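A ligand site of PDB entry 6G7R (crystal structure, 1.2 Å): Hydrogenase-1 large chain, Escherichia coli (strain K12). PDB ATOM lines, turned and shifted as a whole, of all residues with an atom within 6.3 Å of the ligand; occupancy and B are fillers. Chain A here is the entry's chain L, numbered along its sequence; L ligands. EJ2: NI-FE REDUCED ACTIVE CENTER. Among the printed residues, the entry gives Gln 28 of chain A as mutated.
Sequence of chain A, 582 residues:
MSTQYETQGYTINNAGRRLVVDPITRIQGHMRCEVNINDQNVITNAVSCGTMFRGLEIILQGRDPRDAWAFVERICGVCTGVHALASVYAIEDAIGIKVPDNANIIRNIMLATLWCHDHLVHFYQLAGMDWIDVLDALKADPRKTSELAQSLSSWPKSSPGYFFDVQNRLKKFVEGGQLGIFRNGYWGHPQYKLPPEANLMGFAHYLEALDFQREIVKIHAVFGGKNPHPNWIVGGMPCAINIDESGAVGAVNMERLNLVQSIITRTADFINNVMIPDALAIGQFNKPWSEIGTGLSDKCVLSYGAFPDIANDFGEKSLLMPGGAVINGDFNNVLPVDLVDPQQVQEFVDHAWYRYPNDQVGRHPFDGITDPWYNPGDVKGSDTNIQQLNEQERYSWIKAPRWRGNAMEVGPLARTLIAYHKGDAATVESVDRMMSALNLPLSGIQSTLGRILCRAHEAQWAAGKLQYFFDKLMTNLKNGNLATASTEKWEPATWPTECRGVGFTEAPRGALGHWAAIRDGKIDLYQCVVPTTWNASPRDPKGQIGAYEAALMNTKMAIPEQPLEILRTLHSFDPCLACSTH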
ATOM      1  N   GLN A  28      17.990   7.496 -19.742  1.00  0.00           N
ATOM      2  CA  GLN A  28      17.135   8.348 -18.916  1.00  0.00           C
ATOM      3  C   GLN A  28      16.909   7.615 -17.587  1.00  0.00           C
ATOM      4  O   GLN A  28      16.550   6.435 -17.586  1.00  0.00           O
ATOM      5  CB  GLN A  28      15.807   8.684 -19.590  1.00  0.00           C
ATOM      6  CG  GLN A  28      15.024   9.757 -18.828  1.00  0.00           C
ATOM      7  CD  GLN A  28      14.494   9.349 -17.478  1.00  0.00           C
ATOM      8  OE1 GLN A  28      14.153   8.193 -17.282  1.00  0.00           O
ATOM      9  NE2 GLN A  28      14.435  10.287 -16.525  1.00  0.00           N
ATOM     10  N   ILE A  75       5.787  12.086 -16.819  1.00  0.00           N
ATOM     11  CA  ILE A  75       6.464  10.796 -16.696  1.00  0.00           C
ATOM     12  C   ILE A  75       7.862  10.895 -17.287  1.00  0.00           C
ATOM     13  O   ILE A  75       8.780  10.283 -16.751  1.00  0.00           O
ATOM     14  CB  ILE A  75       5.611   9.674 -17.305  1.00  0.00           C
ATOM     15  CG1 ILE A  75       4.398   9.395 -16.417  1.00  0.00           C
ATOM     16  CG2 ILE A  75       6.463   8.414 -17.480  1.00  0.00           C
ATOM     17  CD1 ILE A  75       3.387   8.485 -17.019  1.00  0.00           C
ATOM     18  N   CYS A  76       8.013  11.649 -18.380  1.00  0.00           N
ATOM     19  CA  CYS A  76       9.296  11.616 -19.062  1.00  0.00           C
ATOM     20  C   CYS A  76       9.463  12.855 -19.949  1.00  0.00           C
ATOM     21  O   CYS A  76       8.619  13.178 -20.766  1.00  0.00           O
ATOM     22  CB  CYS A  76       9.418  10.365 -19.924  1.00  0.00           C
ATOM     23  SG  CYS A  76      11.086  10.183 -20.602  1.00  0.00           S
ATOM     24  N   GLY A  77      10.618  13.512 -19.763  1.00  0.00           N
ATOM     25  CA  GLY A  77      11.002  14.676 -20.584  1.00  0.00           C
ATOM     26  C   GLY A  77      11.839  14.329 -21.801  1.00  0.00           C
ATOM     27  O   GLY A  77      12.091  15.218 -22.607  1.00  0.00           O
ATOM     28  N   VAL A  78      12.209  13.055 -21.930  1.00  0.00           N
ATOM     29  CA  VAL A  78      12.941  12.550 -23.091  1.00  0.00           C
ATOM     30  C   VAL A  78      11.910  12.178 -24.154  1.00  0.00           C
ATOM     31  O   VAL A  78      11.883  12.767 -25.247  1.00  0.00           O
ATOM     32  CB  VAL A  78      13.915  11.414 -22.730  1.00  0.00           C
ATOM     33  CG1 VAL A  78      14.629  10.936 -23.973  1.00  0.00           C
ATOM     34  CG2 VAL A  78      14.918  11.881 -21.666  1.00  0.00           C
ATOM     35  N   CYS A  79      11.028  11.256 -23.808  1.00  0.00           N
ATOM     36  CA  CYS A  79       9.899  10.940 -24.676  1.00  0.00           C
ATOM     37  C   CYS A  79       8.744  11.931 -24.432  1.00  0.00           C
ATOM     38  O   CYS A  79       7.586  11.557 -24.233  1.00  0.00           O
ATOM     39  CB  CYS A  79       9.522   9.477 -24.614  1.00  0.00           C
ATOM     40  SG  CYS A  79       9.020   8.851 -22.981  1.00  0.00           S
ATOM     41  N   THR A  80       9.083  13.203 -24.386  1.00  0.00           N
ATOM     42  CA  THR A  80       8.126  14.222 -24.018  1.00  0.00           C
ATOM     43  C   THR A  80       7.039  14.372 -25.101  1.00  0.00           C
ATOM     44  O   THR A  80       7.259  14.550 -26.286  1.00  0.00           O
ATOM     45  CB  THR A  80       8.828  15.562 -23.828  1.00  0.00           C
ATOM     46  OG1 THR A  80       7.854  16.516 -23.399  1.00  0.00           O
ATOM     47  CG2 THR A  80       9.506  16.123 -25.055  1.00  0.00           C
ATOM     48  N   VAL A  82       4.605  11.963 -25.594  1.00  0.00           N
ATOM     49  CA  VAL A  82       3.960  10.705 -25.927  1.00  0.00           C
ATOM     50  C   VAL A  82       2.906  10.343 -24.869  1.00  0.00           C
ATOM     51  O   VAL A  82       1.876   9.749 -25.192  1.00  0.00           O
ATOM     52  CB  VAL A  82       4.934   9.575 -26.237  1.00  0.00           C
ATOM     53  CG1 VAL A  82       5.605   9.026 -24.979  1.00  0.00           C
ATOM     54  CG2 VAL A  82       4.207   8.520 -27.060  1.00  0.00           C
ATOM     55  N   HIS A  83       3.211  10.617 -23.591  1.00  0.00           N
ATOM     56  CA  HIS A  83       2.273  10.306 -22.542  1.00  0.00           C
ATOM     57  C   HIS A  83       1.054  11.212 -22.593  1.00  0.00           C
ATOM     58  O   HIS A  83      -0.033  10.789 -22.231  1.00  0.00           O
ATOM     59  CB  HIS A  83       2.956  10.349 -21.169  1.00  0.00           C
ATOM     60  CG  HIS A  83       3.914   9.245 -20.966  1.00  0.00           C
ATOM     61  ND1 HIS A  83       3.486   7.950 -20.785  1.00  0.00           N
ATOM     62  CD2 HIS A  83       5.273   9.226 -21.002  1.00  0.00           C
ATOM     63  CE1 HIS A  83       4.553   7.203 -20.613  1.00  0.00           C
ATOM     64  NE2 HIS A  83       5.663   7.939 -20.772  1.00  0.00           N
ATOM     65  N   LEU A 114       8.647  13.860 -32.388  1.00  0.00           N
ATOM     66  CA  LEU A 114       9.297  13.228 -31.269  1.00  0.00           C
ATOM     67  C   LEU A 114      10.136  12.019 -31.707  1.00  0.00           C
ATOM     68  O   LEU A 114      11.271  11.854 -31.276  1.00  0.00           O
ATOM     69  CB  LEU A 114       8.277  12.811 -30.208  1.00  0.00           C
ATOM     70  CG  LEU A 114       8.872  12.056 -28.996  1.00  0.00           C
ATOM     71  CD1 LEU A 114       9.836  12.942 -28.207  1.00  0.00           C
ATOM     72  CD2 LEU A 114       7.761  11.483 -28.116  1.00  0.00           C
ATOM     73  N   ASP A 118      13.999  12.136 -30.769  1.00  0.00           N
ATOM     74  CA  ASP A 118      14.419  11.201 -29.754  1.00  0.00           C
ATOM     75  C   ASP A 118      15.397  10.180 -30.348  1.00  0.00           C
ATOM     76  O   ASP A 118      16.463   9.861 -29.770  1.00  0.00           O
ATOM     77  CB  ASP A 118      13.178  10.534 -29.164  1.00  0.00           C
ATOM     78  CG  ASP A 118      13.345   9.920 -27.798  1.00  0.00           C
ATOM     79  OD1 ASP A 118      14.441   9.440 -27.513  1.00  0.00           O
ATOM     80  OD2 ASP A 118      12.305   9.821 -27.054  1.00  0.00           O
ATOM     81  N   ALA A 507       5.449   4.772 -28.701  1.00  0.00           N
ATOM     82  CA  ALA A 507       6.458   5.716 -28.314  1.00  0.00           C
ATOM     83  C   ALA A 507       7.779   5.341 -29.014  1.00  0.00           C
ATOM     84  O   ALA A 507       7.929   4.217 -29.501  1.00  0.00           O
ATOM     85  CB  ALA A 507       6.609   5.701 -26.818  1.00  0.00           C
ATOM     86  N   PRO A 508       8.758   6.241 -28.995  1.00  0.00           N
ATOM     87  CA  PRO A 508      10.064   5.867 -29.568  1.00  0.00           C
ATOM     88  C   PRO A 508      10.603   4.519 -29.093  1.00  0.00           C
ATOM     89  O   PRO A 508      11.197   3.783 -29.876  1.00  0.00           O
ATOM     90  CB  PRO A 508      10.969   7.045 -29.152  1.00  0.00           C
ATOM     91  CG  PRO A 508      10.010   8.226 -29.163  1.00  0.00           C
ATOM     92  CD  PRO A 508       8.739   7.638 -28.576  1.00  0.00           C
ATOM     93  N   ARG A 509      10.371   4.190 -27.825  1.00  0.00           N
ATOM     94  CA  ARG A 509      10.911   2.939 -27.246  1.00  0.00           C
ATOM     95  C   ARG A 509       9.981   1.729 -27.318  1.00  0.00           C
ATOM     96  O   ARG A 509      10.432   0.637 -26.977  1.00  0.00           O
ATOM     97  CB  ARG A 509      11.342   3.230 -25.808  1.00  0.00           C
ATOM     98  CG  ARG A 509      12.549   4.164 -25.782  1.00  0.00           C
ATOM     99  CD  ARG A 509      12.731   4.862 -24.484  1.00  0.00           C
ATOM    100  NE  ARG A 509      13.783   5.854 -24.529  1.00  0.00           N
ATOM    101  CZ  ARG A 509      13.706   7.045 -25.121  1.00  0.00           C
ATOM    102  NH1 ARG A 509      12.548   7.543 -25.511  1.00  0.00           N
ATOM    103  NH2 ARG A 509      14.783   7.795 -25.223  1.00  0.00           N
ATOM    104  N   GLY A 510       8.743   1.920 -27.801  1.00  0.00           N
ATOM    105  CA  GLY A 510       7.848   0.795 -27.971  1.00  0.00           C
ATOM    106  C   GLY A 510       6.410   1.066 -27.554  1.00  0.00           C
ATOM    107  O   GLY A 510       5.957   2.186 -27.457  1.00  0.00           O
ATOM    108  N   ALA A 511       5.680  -0.015 -27.329  1.00  0.00           N
ATOM    109  CA  ALA A 511       4.238  -0.027 -27.105  1.00  0.00           C
ATOM    110  C   ALA A 511       3.877   0.642 -25.777  1.00  0.00           C
ATOM    111  O   ALA A 511       4.317   0.208 -24.713  1.00  0.00           O
ATOM    112  CB  ALA A 511       3.760  -1.447 -27.091  1.00  0.00           C
ATOM    113  N   LEU A 512       3.034   1.696 -25.858  1.00  0.00           N
ATOM    114  CA  LEU A 512       2.595   2.457 -24.690  1.00  0.00           C
ATOM    115  C   LEU A 512       1.085   2.340 -24.547  1.00  0.00           C
ATOM    116  O   LEU A 512       0.362   2.572 -25.534  1.00  0.00           O
ATOM    117  CB  LEU A 512       2.994   3.921 -24.891  1.00  0.00           C
ATOM    118  CG  LEU A 512       2.442   4.912 -23.861  1.00  0.00           C
ATOM    119  CD1 LEU A 512       2.929   4.588 -22.456  1.00  0.00           C
ATOM    120  CD2 LEU A 512       2.789   6.326 -24.250  1.00  0.00           C
ATOM    121  N   VAL A 530       4.362   1.000 -19.886  1.00  0.00           N
ATOM    122  CA  VAL A 530       5.167   1.845 -20.748  1.00  0.00           C
ATOM    123  C   VAL A 530       6.224   0.964 -21.407  1.00  0.00           C
ATOM    124  O   VAL A 530       6.544  -0.101 -20.898  1.00  0.00           O
ATOM    125  CB  VAL A 530       5.729   2.984 -19.870  1.00  0.00           C
ATOM    126  CG1 VAL A 530       6.538   3.989 -20.595  1.00  0.00           C
ATOM    127  CG2 VAL A 530       4.617   3.668 -19.096  1.00  0.00           C
ATOM    128  N   PRO A 531       6.798   1.369 -22.544  1.00  0.00           N
ATOM    129  CA  PRO A 531       7.668   0.437 -23.256  1.00  0.00           C
ATOM    130  C   PRO A 531       8.833  -0.113 -22.430  1.00  0.00           C
ATOM    131  O   PRO A 531       9.103  -1.299 -22.470  1.00  0.00           O
ATOM    132  CB  PRO A 531       8.157   1.198 -24.497  1.00  0.00           C
ATOM    133  CG  PRO A 531       7.428   2.474 -24.503  1.00  0.00           C
ATOM    134  CD  PRO A 531       6.411   2.467 -23.411  1.00  0.00           C
ATOM    135  N   THR A 532       9.541   0.741 -21.718  1.00  0.00           N
ATOM    136  CA  THR A 532      10.666   0.251 -20.907  1.00  0.00           C
ATOM    137  C   THR A 532      10.143  -0.625 -19.752  1.00  0.00           C
ATOM    138  O   THR A 532      10.909  -1.461 -19.237  1.00  0.00           O
ATOM    139  CB  THR A 532      11.600   1.394 -20.513  1.00  0.00           C
ATOM    140  OG1 THR A 532      12.090   2.029 -21.701  1.00  0.00           O
ATOM    141  CG2 THR A 532      12.778   0.924 -19.697  1.00  0.00           C
ATOM    142  N   THR A 533       8.878  -0.477 -19.325  1.00  0.00           N
ATOM    143  CA  THR A 533       8.330  -1.425 -18.362  1.00  0.00           C
ATOM    144  C   THR A 533       8.414  -2.865 -18.919  1.00  0.00           C
ATOM    145  O   THR A 533       8.806  -3.796 -18.228  1.00  0.00           O
ATOM    146  CB  THR A 533       6.884  -1.112 -17.976  1.00  0.00           C
ATOM    147  OG1 THR A 533       6.686   0.291 -17.763  1.00  0.00           O
ATOM    148  CG2 THR A 533       6.457  -1.887 -16.741  1.00  0.00           C
ATOM    149  N   ASP A 574      17.541   1.712 -25.793  1.00  0.00           N
ATOM    150  CA  ASP A 574      17.211   3.096 -25.405  1.00  0.00           C
ATOM    151  C   ASP A 574      16.389   3.136 -24.103  1.00  0.00           C
ATOM    152  O   ASP A 574      15.242   3.567 -24.056  1.00  0.00           O
ATOM    153  CB  ASP A 574      16.520   3.739 -26.598  1.00  0.00           C
ATOM    154  CG  ASP A 574      16.244   5.192 -26.468  1.00  0.00           C
ATOM    155  OD1 ASP A 574      16.728   5.814 -25.511  1.00  0.00           O
ATOM    156  OD2 ASP A 574      15.561   5.715 -27.390  1.00  0.00           O
ATOM    157  N   PRO A 575      16.988   2.672 -23.010  1.00  0.00           N
ATOM    158  CA  PRO A 575      16.213   2.568 -21.765  1.00  0.00           C
ATOM    159  C   PRO A 575      15.723   3.936 -21.253  1.00  0.00           C
ATOM    160  O   PRO A 575      16.500   4.911 -21.230  1.00  0.00           O
ATOM    161  CB  PRO A 575      17.165   1.940 -20.725  1.00  0.00           C
ATOM    162  CG  PRO A 575      18.202   1.239 -21.584  1.00  0.00           C
ATOM    163  CD  PRO A 575      18.329   2.113 -22.821  1.00  0.00           C
ATOM    164  N   CYS A 576      14.461   3.971 -20.837  1.00  0.00           N
ATOM    165  CA  CYS A 576      13.902   5.136 -20.220  1.00  0.00           C
ATOM    166  C   CYS A 576      13.328   4.727 -18.864  1.00  0.00           C
ATOM    167  O   CYS A 576      12.217   4.159 -18.800  1.00  0.00           O
ATOM    168  CB  CYS A 576      12.861   5.790 -21.117  1.00  0.00           C
ATOM    169  SG  CYS A 576      12.350   7.377 -20.447  1.00  0.00           S
ATOM    170  N   LEU A 577      14.084   4.957 -17.808  1.00  0.00           N
ATOM    171  CA  LEU A 577      13.724   4.367 -16.537  1.00  0.00           C
ATOM    172  C   LEU A 577      12.622   5.150 -15.831  1.00  0.00           C
ATOM    173  O   LEU A 577      11.827   4.537 -15.098  1.00  0.00           O
ATOM    174  CB  LEU A 577      14.958   4.194 -15.662  1.00  0.00           C
ATOM    175  CG  LEU A 577      15.750   2.913 -15.939  1.00  0.00           C
ATOM    176  CD1 LEU A 577      15.027   1.698 -15.395  1.00  0.00           C
ATOM    177  CD2 LEU A 577      16.087   2.713 -17.412  1.00  0.00           C
ATOM    178  N   ALA A 578      12.530   6.467 -16.043  1.00  0.00           N
ATOM    179  CA  ALA A 578      11.417   7.231 -15.493  1.00  0.00           C
ATOM    180  C   ALA A 578      10.126   6.750 -16.149  1.00  0.00           C
ATOM    181  O   ALA A 578       9.086   6.609 -15.472  1.00  0.00           O
ATOM    182  CB  ALA A 578      11.617   8.704 -15.692  1.00  0.00           C
ATOM    183  N   CYS A 579      10.162   6.505 -17.449  1.00  0.00           N
ATOM    184  CA  CYS A 579       9.016   5.904 -18.111  1.00  0.00           C
ATOM    185  C   CYS A 579       8.663   4.545 -17.494  1.00  0.00           C
ATOM    186  O   CYS A 579       7.485   4.261 -17.300  1.00  0.00           O
ATOM    187  CB  CYS A 579       9.305   5.678 -19.594  1.00  0.00           C
ATOM    188  SG  CYS A 579       8.844   7.066 -20.632  1.00  0.00           S
ATOM    189  N   SER A 580       9.681   3.716 -17.242  1.00  0.00           N
ATOM    190  CA  SER A 580       9.413   2.346 -16.862  1.00  0.00           C
ATOM    191  C   SER A 580       8.687   2.235 -15.519  1.00  0.00           C
ATOM    192  O   SER A 580       7.909   1.292 -15.324  1.00  0.00           O
ATOM    193  CB  SER A 580      10.680   1.556 -16.817  1.00  0.00           C
ATOM    194  OG  SER A 580      11.463   1.815 -15.671  1.00  0.00           O
HETATM  195 FE   EJ2 L   1       9.083   6.580 -22.870  1.00  0.00          FE
HETATM  196 NI   EJ2 L   1      10.780   8.210 -21.648  1.00  0.00          NI
HETATM  197  C1  EJ2 L   1       9.567   4.820 -22.536  1.00  0.00           C
HETATM  198  N1  EJ2 L   1       9.889   3.728 -22.286  1.00  0.00           N
HETATM  199  C2  EJ2 L   1       9.471   6.345 -24.683  1.00  0.00           C
HETATM  200  N2  EJ2 L   1       9.758   6.188 -25.806  1.00  0.00           N
HETATM  201  C3  EJ2 L   1       7.401   6.164 -23.219  1.00  0.00           C
HETATM  202  O3  EJ2 L   1       6.339   5.897 -23.414  1.00  0.00           O
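NI of the ligand is bound by SG of Cys 576. The side-chain sulfur (SG) of Cys 76 binds a nickel atom (NI) of the ligand, at 2.3 Å. The side-chain sulfur (SG) of Cys 79 is bound to an iron atom (FE) of the ligand (2.3 Å). SG of Cys 579 binds FE of the ligand (2.3 Å). The backbone NH of Thr 532 lies within hydrogen-bond range of a nitrogen (N1) of the ligand, at 3.1 Å. OG1 of Thr 532 is in hydrogen-bond range of N1 of the ligand, 2.8 Å away. N of Arg 509 lies within hydrogen-bond range of N2 of the ligand (2.9 Å). The guanidinium group of Arg 509 lies within hydrogen-bond range of a nitrogen (N2) of the ligand (3.1 Å). A ring nitrogen (NE2) of His 83 lies within hydrogen-bond range of an oxygen (O3) of the ligand, 3.4 Å away.
The backbone NH of Cys 576 sits at hydrogen-bond distance from the side-chain hydroxyl of Thr 532 (3.2 Å). The side-chain amide oxygen (OE1) of Gln 28 lies close to the side-chain sulfur (SG) of Cys 576 (3.7 Å). The side-chain sulfur of Cys 76 lies close to the backbone NH of Val 78 (3.4 Å). SG of Cys 579 lies close to NE2 of His 83 (3.3 Å). OD2 of Asp 118 lies within salt-bridge range of NH1 of Arg 509, at 2.8 Å. The guanidinium group (NH2) of Arg 509 lies within salt-bridge range of the side-chain carboxylate (OD1) of Asp 574 (2.8 Å). OG1 of Thr 533 sits close to O of Val 530, at 3.2 Å.
The backbone nitrogen of Pro 508 lies close to a nitrogen (N2) of the ligand. Residues that only touch the ligand: Ala 507, Val 530, Pro 531, Val 82 and Leu 512. Hydrophobic or aromatic side chains that line the ligand: Val 82, His 83, Ala 507, Pro 508, Leu 512, Val 530 and Pro 531. 13 residues have an atom within 4 Å of the ligand: Cys 76, Cys 79, Val 82, His 83, Ala 507, Pro 508, Arg 509, Leu 512, Val 530, Pro 531, Thr 532, Cys 576 and Cys 579.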
